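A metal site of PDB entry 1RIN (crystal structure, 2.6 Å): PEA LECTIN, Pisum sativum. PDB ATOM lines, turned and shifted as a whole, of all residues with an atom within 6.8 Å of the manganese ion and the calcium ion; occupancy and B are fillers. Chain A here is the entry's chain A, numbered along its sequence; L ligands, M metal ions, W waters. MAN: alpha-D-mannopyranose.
The manganese ion is bound by water W3, the side-chain carboxylate (OD2) of Asp 121, water W1, the side-chain carboxylate (OE2) of Glu 119, the side-chain carboxylate (OD1) of Asp 129 and a ring nitrogen (NE2) of His 136.
Of the 23 residues printed, 4 come within 4 Å of the calcium ion.
The nearest printed residue that does not touch the calcium ion is Trp 128 (4.4 Å).
The calcium ion is bound by the backbone carbonyl oxygen (O) of Phe 123 (2.3 Å), the side-chain carboxylate (OD2) of Asp 129 (2.3 Å), the side-chain carboxylate (OD1) of Asp 121 (2.3 Å), water W4 (2.4 Å), water W2 (2.4 Å), the side-chain carboxylate (OD2) of Asp 121 (2.4 Å) and the side-chain amide oxygen (OD1) of Asn 125 (2.5 Å).
The calcium ion has seven donor atoms within binding distance.
An oxygen (O4) of the ligand lies within hydrogen-bond range of the side-chain amide nitrogen (ND2) of Asn 125, 2.9 Å away.
An oxygen (O3) of the ligand lies within hydrogen-bond range of the backbone NH (N) of Gly 99.
The side-chain carboxylate (OD1) of Asp 81 is in hydrogen-bond range of an oxygen (O4) of the ligand.
Within 4 Å of the manganese ion: Glu 119, Asp 121, Asp 129 and His 136.
The backbone NH of Glu 119 is in hydrogen-bond range of the backbone carbonyl oxygen of Gly 138, 2.9 Å away.
The indole nitrogen of Trp 128 sits close to the side-chain carboxylate of Asp 129 (3.3 Å).
Water W3 lies within hydrogen-bond range of the side-chain carboxylate of Glu 119 (2.6 Å) and the backbone carbonyl oxygen of Ile 144 (2.9 Å).
Water W2 lies within hydrogen-bond range of NE1 of Trp 128 (2.8 Å) and O of Gly 99 (2.8 Å).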
ATOM      1  N   ASP A  81      -4.247 -23.367  32.364  1.00  0.00           N
ATOM      2  CA  ASP A  81      -4.449 -22.726  31.090  1.00  0.00           C
ATOM      3  C   ASP A  81      -4.272 -21.222  31.130  1.00  0.00           C
ATOM      4  O   ASP A  81      -3.829 -20.577  30.169  1.00  0.00           O
ATOM      5  CB  ASP A  81      -5.788 -23.001  30.635  1.00  0.00           C
ATOM      6  CG  ASP A  81      -5.663 -24.221  29.735  1.00  0.00           C
ATOM      7  OD1 ASP A  81      -5.360 -24.106  28.572  1.00  0.00           O
ATOM      8  OD2 ASP A  81      -5.871 -25.355  30.177  1.00  0.00           O
ATOM      9  N   GLY A  98     -10.742 -25.227  29.886  1.00  0.00           N
ATOM     10  CA  GLY A  98      -9.423 -25.476  29.343  1.00  0.00           C
ATOM     11  C   GLY A  98      -8.853 -24.289  28.572  1.00  0.00           C
ATOM     12  O   GLY A  98      -8.767 -23.163  29.073  1.00  0.00           O
ATOM     13  N   GLY A  99      -8.602 -24.449  27.282  1.00  0.00           N
ATOM     14  CA  GLY A  99      -7.976 -23.409  26.498  1.00  0.00           C
ATOM     15  C   GLY A  99      -8.828 -22.187  26.293  1.00  0.00           C
ATOM     16  O   GLY A  99      -8.312 -21.165  25.879  1.00  0.00           O
ATOM     17  N   TYR A 100     -10.139 -22.251  26.554  1.00  0.00           N
ATOM     18  CA  TYR A 100     -11.013 -21.074  26.350  1.00  0.00           C
ATOM     19  C   TYR A 100     -11.206 -20.195  27.573  1.00  0.00           C
ATOM     20  O   TYR A 100     -12.022 -19.267  27.595  1.00  0.00           O
ATOM     21  CB  TYR A 100     -12.379 -21.501  25.862  1.00  0.00           C
ATOM     22  CG  TYR A 100     -12.308 -22.147  24.495  1.00  0.00           C
ATOM     23  CD1 TYR A 100     -12.271 -21.363  23.364  1.00  0.00           C
ATOM     24  CD2 TYR A 100     -12.280 -23.508  24.403  1.00  0.00           C
ATOM     25  CE1 TYR A 100     -12.204 -21.938  22.125  1.00  0.00           C
ATOM     26  CE2 TYR A 100     -12.219 -24.095  23.161  1.00  0.00           C
ATOM     27  CZ  TYR A 100     -12.183 -23.311  22.030  1.00  0.00           C
ATOM     28  OH  TYR A 100     -12.109 -23.898  20.790  1.00  0.00           O
ATOM     29  N   LEU A 101     -10.443 -20.491  28.628  1.00  0.00           N
ATOM     30  CA  LEU A 101     -10.351 -19.687  29.851  1.00  0.00           C
ATOM     31  C   LEU A 101     -11.660 -19.411  30.601  1.00  0.00           C
ATOM     32  O   LEU A 101     -11.699 -18.677  31.602  1.00  0.00           O
ATOM     33  CB  LEU A 101      -9.614 -18.349  29.496  1.00  0.00           C
ATOM     34  CG  LEU A 101      -8.238 -18.467  28.793  1.00  0.00           C
ATOM     35  CD1 LEU A 101      -7.673 -17.112  28.442  1.00  0.00           C
ATOM     36  CD2 LEU A 101      -7.263 -19.180  29.703  1.00  0.00           C
ATOM     37  N   GLU A 119      -6.344 -11.579  28.814  1.00  0.00           N
ATOM     38  CA  GLU A 119      -5.848 -12.876  29.258  1.00  0.00           C
ATOM     39  C   GLU A 119      -4.384 -12.917  29.638  1.00  0.00           C
ATOM     40  O   GLU A 119      -3.572 -12.116  29.175  1.00  0.00           O
ATOM     41  CB  GLU A 119      -6.059 -13.912  28.206  1.00  0.00           C
ATOM     42  CG  GLU A 119      -5.282 -13.604  26.930  1.00  0.00           C
ATOM     43  CD  GLU A 119      -5.293 -14.715  25.912  1.00  0.00           C
ATOM     44  OE1 GLU A 119      -6.358 -15.158  25.554  1.00  0.00           O
ATOM     45  OE2 GLU A 119      -4.226 -15.122  25.487  1.00  0.00           O
ATOM     46  N   PHE A 120      -4.061 -13.841  30.512  1.00  0.00           N
ATOM     47  CA  PHE A 120      -2.703 -14.139  30.931  1.00  0.00           C
ATOM     48  C   PHE A 120      -2.621 -15.638  30.657  1.00  0.00           C
ATOM     49  O   PHE A 120      -3.028 -16.506  31.449  1.00  0.00           O
ATOM     50  CB  PHE A 120      -2.517 -13.794  32.432  1.00  0.00           C
ATOM     51  CG  PHE A 120      -2.794 -12.307  32.708  1.00  0.00           C
ATOM     52  CD1 PHE A 120      -1.808 -11.350  32.527  1.00  0.00           C
ATOM     53  CD2 PHE A 120      -4.061 -11.898  33.089  1.00  0.00           C
ATOM     54  CE1 PHE A 120      -2.128 -10.012  32.691  1.00  0.00           C
ATOM     55  CE2 PHE A 120      -4.364 -10.557  33.239  1.00  0.00           C
ATOM     56  CZ  PHE A 120      -3.391  -9.607  33.048  1.00  0.00           C
ATOM     57  N   ASP A 121      -2.213 -15.940  29.437  1.00  0.00           N
ATOM     58  CA  ASP A 121      -2.263 -17.288  28.897  1.00  0.00           C
ATOM     59  C   ASP A 121      -0.941 -18.039  29.060  1.00  0.00           C
ATOM     60  O   ASP A 121       0.123 -17.653  28.558  1.00  0.00           O
ATOM     61  CB  ASP A 121      -2.664 -17.155  27.433  1.00  0.00           C
ATOM     62  CG  ASP A 121      -3.008 -18.410  26.640  1.00  0.00           C
ATOM     63  OD1 ASP A 121      -2.568 -19.499  27.017  1.00  0.00           O
ATOM     64  OD2 ASP A 121      -3.726 -18.319  25.631  1.00  0.00           O
ATOM     65  N   THR A 122      -1.019 -19.179  29.759  1.00  0.00           N
ATOM     66  CA  THR A 122       0.164 -19.976  30.070  1.00  0.00           C
ATOM     67  C   THR A 122       0.377 -21.220  29.193  1.00  0.00           C
ATOM     68  O   THR A 122       1.408 -21.892  29.220  1.00  0.00           O
ATOM     69  CB  THR A 122       0.136 -20.423  31.519  1.00  0.00           C
ATOM     70  OG1 THR A 122      -1.088 -21.093  31.716  1.00  0.00           O
ATOM     71  CG2 THR A 122       0.211 -19.282  32.499  1.00  0.00           C
ATOM     72  N   PHE A 123      -0.576 -21.488  28.300  1.00  0.00           N
ATOM     73  CA  PHE A 123      -0.547 -22.688  27.511  1.00  0.00           C
ATOM     74  C   PHE A 123      -0.767 -22.404  26.057  1.00  0.00           C
ATOM     75  O   PHE A 123      -1.750 -21.759  25.685  1.00  0.00           O
ATOM     76  CB  PHE A 123      -1.633 -23.659  27.958  1.00  0.00           C
ATOM     77  CG  PHE A 123      -1.505 -25.046  27.323  1.00  0.00           C
ATOM     78  CD1 PHE A 123      -0.662 -25.986  27.901  1.00  0.00           C
ATOM     79  CD2 PHE A 123      -2.259 -25.352  26.203  1.00  0.00           C
ATOM     80  CE1 PHE A 123      -0.573 -27.254  27.354  1.00  0.00           C
ATOM     81  CE2 PHE A 123      -2.169 -26.603  25.653  1.00  0.00           C
ATOM     82  CZ  PHE A 123      -1.317 -27.545  26.220  1.00  0.00           C
ATOM     83  N   TYR A 124       0.121 -22.952  25.204  1.00  0.00           N
ATOM     84  CA  TYR A 124       0.011 -22.730  23.771  1.00  0.00           C
ATOM     85  C   TYR A 124      -1.030 -23.666  23.178  1.00  0.00           C
ATOM     86  O   TYR A 124      -0.955 -24.889  23.268  1.00  0.00           O
ATOM     87  CB  TYR A 124       1.422 -22.936  23.107  1.00  0.00           C
ATOM     88  CG  TYR A 124       1.402 -22.878  21.581  1.00  0.00           C
ATOM     89  CD1 TYR A 124       1.191 -21.682  20.903  1.00  0.00           C
ATOM     90  CD2 TYR A 124       1.518 -24.066  20.879  1.00  0.00           C
ATOM     91  CE1 TYR A 124       1.088 -21.703  19.523  1.00  0.00           C
ATOM     92  CE2 TYR A 124       1.414 -24.086  19.500  1.00  0.00           C
ATOM     93  CZ  TYR A 124       1.199 -22.903  18.848  1.00  0.00           C
ATOM     94  OH  TYR A 124       1.071 -22.955  17.483  1.00  0.00           O
ATOM     95  N   ASN A 125      -2.033 -23.084  22.562  1.00  0.00           N
ATOM     96  CA  ASN A 125      -3.041 -23.823  21.839  1.00  0.00           C
ATOM     97  C   ASN A 125      -2.841 -23.513  20.368  1.00  0.00           C
ATOM     98  O   ASN A 125      -3.133 -22.414  19.869  1.00  0.00           O
ATOM     99  CB  ASN A 125      -4.465 -23.405  22.218  1.00  0.00           C
ATOM    100  CG  ASN A 125      -4.825 -23.673  23.668  1.00  0.00           C
ATOM    101  OD1 ASN A 125      -4.809 -22.733  24.444  1.00  0.00           O
ATOM    102  ND2 ASN A 125      -5.172 -24.848  24.164  1.00  0.00           N
ATOM    103  N   TRP A 128      -5.021 -21.075  17.738  1.00  0.00           N
ATOM    104  CA  TRP A 128      -5.247 -19.614  17.829  1.00  0.00           C
ATOM    105  C   TRP A 128      -4.144 -18.863  18.582  1.00  0.00           C
ATOM    106  O   TRP A 128      -4.009 -17.657  18.435  1.00  0.00           O
ATOM    107  CB  TRP A 128      -6.598 -19.303  18.536  1.00  0.00           C
ATOM    108  CG  TRP A 128      -6.765 -19.923  19.930  1.00  0.00           C
ATOM    109  CD1 TRP A 128      -6.088 -19.397  20.982  1.00  0.00           C
ATOM    110  CD2 TRP A 128      -7.483 -21.056  20.289  1.00  0.00           C
ATOM    111  NE1 TRP A 128      -6.327 -20.174  21.992  1.00  0.00           N
ATOM    112  CE2 TRP A 128      -7.149 -21.179  21.632  1.00  0.00           C
ATOM    113  CE3 TRP A 128      -8.328 -22.004  19.720  1.00  0.00           C
ATOM    114  CZ2 TRP A 128      -7.658 -22.209  22.407  1.00  0.00           C
ATOM    115  CZ3 TRP A 128      -8.837 -23.035  20.495  1.00  0.00           C
ATOM    116  CH2 TRP A 128      -8.500 -23.131  21.825  1.00  0.00           C
ATOM    117  N   ASP A 129      -3.310 -19.552  19.391  1.00  0.00           N
ATOM    118  CA  ASP A 129      -2.272 -18.862  20.142  1.00  0.00           C
ATOM    119  C   ASP A 129      -1.030 -18.481  19.331  1.00  0.00           C
ATOM    120  O   ASP A 129      -0.701 -19.184  18.364  1.00  0.00           O
ATOM    121  CB  ASP A 129      -1.878 -19.716  21.344  1.00  0.00           C
ATOM    122  CG  ASP A 129      -2.816 -19.565  22.538  1.00  0.00           C
ATOM    123  OD1 ASP A 129      -3.484 -18.552  22.680  1.00  0.00           O
ATOM    124  OD2 ASP A 129      -2.866 -20.462  23.378  1.00  0.00           O
ATOM    125  N   PRO A 130      -0.280 -17.429  19.704  1.00  0.00           N
ATOM    126  CA  PRO A 130       0.907 -16.962  18.986  1.00  0.00           C
ATOM    127  C   PRO A 130       1.927 -18.016  18.612  1.00  0.00           C
ATOM    128  O   PRO A 130       2.372 -18.842  19.413  1.00  0.00           O
ATOM    129  CB  PRO A 130       1.527 -15.914  19.858  1.00  0.00           C
ATOM    130  CG  PRO A 130       0.425 -15.448  20.741  1.00  0.00           C
ATOM    131  CD  PRO A 130      -0.345 -16.733  20.992  1.00  0.00           C
ATOM    132  N   HIS A 136       1.888 -15.475  27.201  1.00  0.00           N
ATOM    133  CA  HIS A 136       1.651 -14.128  26.754  1.00  0.00           C
ATOM    134  C   HIS A 136       0.502 -13.433  27.433  1.00  0.00           C
ATOM    135  O   HIS A 136      -0.378 -14.038  28.044  1.00  0.00           O
ATOM    136  CB  HIS A 136       1.418 -14.156  25.204  1.00  0.00           C
ATOM    137  CG  HIS A 136       0.293 -15.091  24.775  1.00  0.00           C
ATOM    138  ND1 HIS A 136       0.444 -16.397  24.641  1.00  0.00           N
ATOM    139  CD2 HIS A 136      -1.029 -14.760  24.543  1.00  0.00           C
ATOM    140  CE1 HIS A 136      -0.715 -16.906  24.370  1.00  0.00           C
ATOM    141  NE2 HIS A 136      -1.602 -15.915  24.302  1.00  0.00           N
ATOM    142  N   ILE A 137       0.521 -12.125  27.352  1.00  0.00           N
ATOM    143  CA  ILE A 137      -0.589 -11.268  27.718  1.00  0.00           C
ATOM    144  C   ILE A 137      -1.384 -11.076  26.446  1.00  0.00           C
ATOM    145  O   ILE A 137      -0.809 -11.104  25.353  1.00  0.00           O
ATOM    146  CB  ILE A 137      -0.070  -9.915  28.241  1.00  0.00           C
ATOM    147  CG1 ILE A 137       0.765 -10.133  29.486  1.00  0.00           C
ATOM    148  CG2 ILE A 137      -1.219  -9.009  28.637  1.00  0.00           C
ATOM    149  CD1 ILE A 137       1.495  -8.870  29.970  1.00  0.00           C
ATOM    150  N   GLY A 138      -2.687 -10.929  26.516  1.00  0.00           N
ATOM    151  CA  GLY A 138      -3.462 -10.673  25.310  1.00  0.00           C
ATOM    152  C   GLY A 138      -4.766  -9.909  25.530  1.00  0.00           C
ATOM    153  O   GLY A 138      -5.375  -9.923  26.605  1.00  0.00           O
ATOM    154  N   ASP A 140      -8.579  -9.789  24.304  1.00  0.00           N
ATOM    155  CA  ASP A 140      -9.569 -10.584  23.599  1.00  0.00           C
ATOM    156  C   ASP A 140     -10.939  -9.931  23.401  1.00  0.00           C
ATOM    157  O   ASP A 140     -11.642  -9.544  24.331  1.00  0.00           O
ATOM    158  CB  ASP A 140      -9.819 -11.912  24.312  1.00  0.00           C
ATOM    159  CG  ASP A 140      -8.689 -12.903  24.515  1.00  0.00           C
ATOM    160  OD1 ASP A 140      -7.620 -12.755  23.943  1.00  0.00           O
ATOM    161  OD2 ASP A 140      -8.890 -13.863  25.256  1.00  0.00           O
ATOM    162  N   ILE A 144     -11.421 -16.242  21.361  1.00  0.00           N
ATOM    163  CA  ILE A 144     -10.272 -16.623  22.178  1.00  0.00           C
ATOM    164  C   ILE A 144      -8.956 -16.334  21.431  1.00  0.00           C
ATOM    165  O   ILE A 144      -7.854 -16.401  21.967  1.00  0.00           O
ATOM    166  CB  ILE A 144     -10.424 -18.113  22.564  1.00  0.00           C
ATOM    167  CG1 ILE A 144      -9.385 -18.465  23.628  1.00  0.00           C
ATOM    168  CG2 ILE A 144     -10.284 -19.015  21.359  1.00  0.00           C
ATOM    169  CD1 ILE A 144      -9.463 -17.648  24.931  1.00  0.00           C
ATOM    170  N   LYS A 145      -9.067 -15.968  20.166  1.00  0.00           N
ATOM    171  CA  LYS A 145      -7.918 -15.560  19.403  1.00  0.00           C
ATOM    172  C   LYS A 145      -7.713 -14.066  19.588  1.00  0.00           C
ATOM    173  O   LYS A 145      -8.440 -13.248  19.023  1.00  0.00           O
ATOM    174  CB  LYS A 145      -8.132 -15.908  17.945  1.00  0.00           C
ATOM    175  CG  LYS A 145      -6.861 -15.658  17.161  1.00  0.00           C
ATOM    176  CD  LYS A 145      -6.981 -16.376  15.858  1.00  0.00           C
ATOM    177  CE  LYS A 145      -6.691 -15.340  14.800  1.00  0.00           C
ATOM    178  NZ  LYS A 145      -6.359 -15.992  13.545  1.00  0.00           N
ATOM    179  N   SER A 146      -6.766 -13.709  20.446  1.00  0.00           N
ATOM    180  CA  SER A 146      -6.534 -12.314  20.798  1.00  0.00           C
ATOM    181  C   SER A 146      -6.256 -11.313  19.673  1.00  0.00           C
ATOM    182  O   SER A 146      -5.477 -11.577  18.739  1.00  0.00           O
ATOM    183  CB  SER A 146      -5.361 -12.144  21.736  1.00  0.00           C
ATOM    184  OG  SER A 146      -5.130 -13.218  22.625  1.00  0.00           O
ATOM    185  N   THR A 149      -1.211  -9.466  21.405  1.00  0.00           N
ATOM    186  CA  THR A 149      -0.512 -10.197  22.474  1.00  0.00           C
ATOM    187  C   THR A 149       0.916  -9.700  22.764  1.00  0.00           C
ATOM    188  O   THR A 149       1.530  -8.937  22.008  1.00  0.00           O
ATOM    189  CB  THR A 149      -0.323 -11.684  22.201  1.00  0.00           C
ATOM    190  OG1 THR A 149       0.560 -11.774  21.096  1.00  0.00           O
ATOM    191  CG2 THR A 149      -1.620 -12.418  21.945  1.00  0.00           C
HETATM  192  C1  MAN L   1      -6.233 -30.040  26.755  1.00  0.00           C
HETATM  193  C2  MAN L   1      -7.464 -29.160  26.496  1.00  0.00           C
HETATM  194  C3  MAN L   1      -7.015 -27.763  26.114  1.00  0.00           C
HETATM  195  C4  MAN L   1      -6.165 -27.215  27.210  1.00  0.00           C
HETATM  196  C5  MAN L   1      -5.005 -28.152  27.461  1.00  0.00           C
HETATM  197  C6  MAN L   1      -4.127 -27.663  28.593  1.00  0.00           C
HETATM  198  O1  MAN L   1      -5.429 -30.244  25.585  1.00  0.00           O
HETATM  199  O2  MAN L   1      -8.332 -29.136  27.629  1.00  0.00           O
HETATM  200  O3  MAN L   1      -8.102 -26.906  25.840  1.00  0.00           O
HETATM  201  O4  MAN L   1      -5.677 -25.967  26.831  1.00  0.00           O
HETATM  202  O5  MAN L   1      -5.483 -29.441  27.812  1.00  0.00           O
HETATM  203  O6  MAN L   1      -4.704 -27.832  29.852  1.00  0.00           O
HETATM  204 MN    MN M   1      -3.751 -16.800  24.109  1.00  0.00          MN
HETATM  205 CA    CA M   2      -3.761 -20.753  25.483  1.00  0.00          CA
HETATM  206  O   HOH W   1      -3.959 -15.579  22.294  1.00  0.00           O
HETATM  207  O   HOH W   2      -5.963 -20.066  24.717  1.00  0.00           O
HETATM  208  O   HOH W   3      -5.784 -17.115  23.914  1.00  0.00           O
HETATM  209  O   HOH W   4      -4.281 -21.759  27.590  1.00  0.00           O
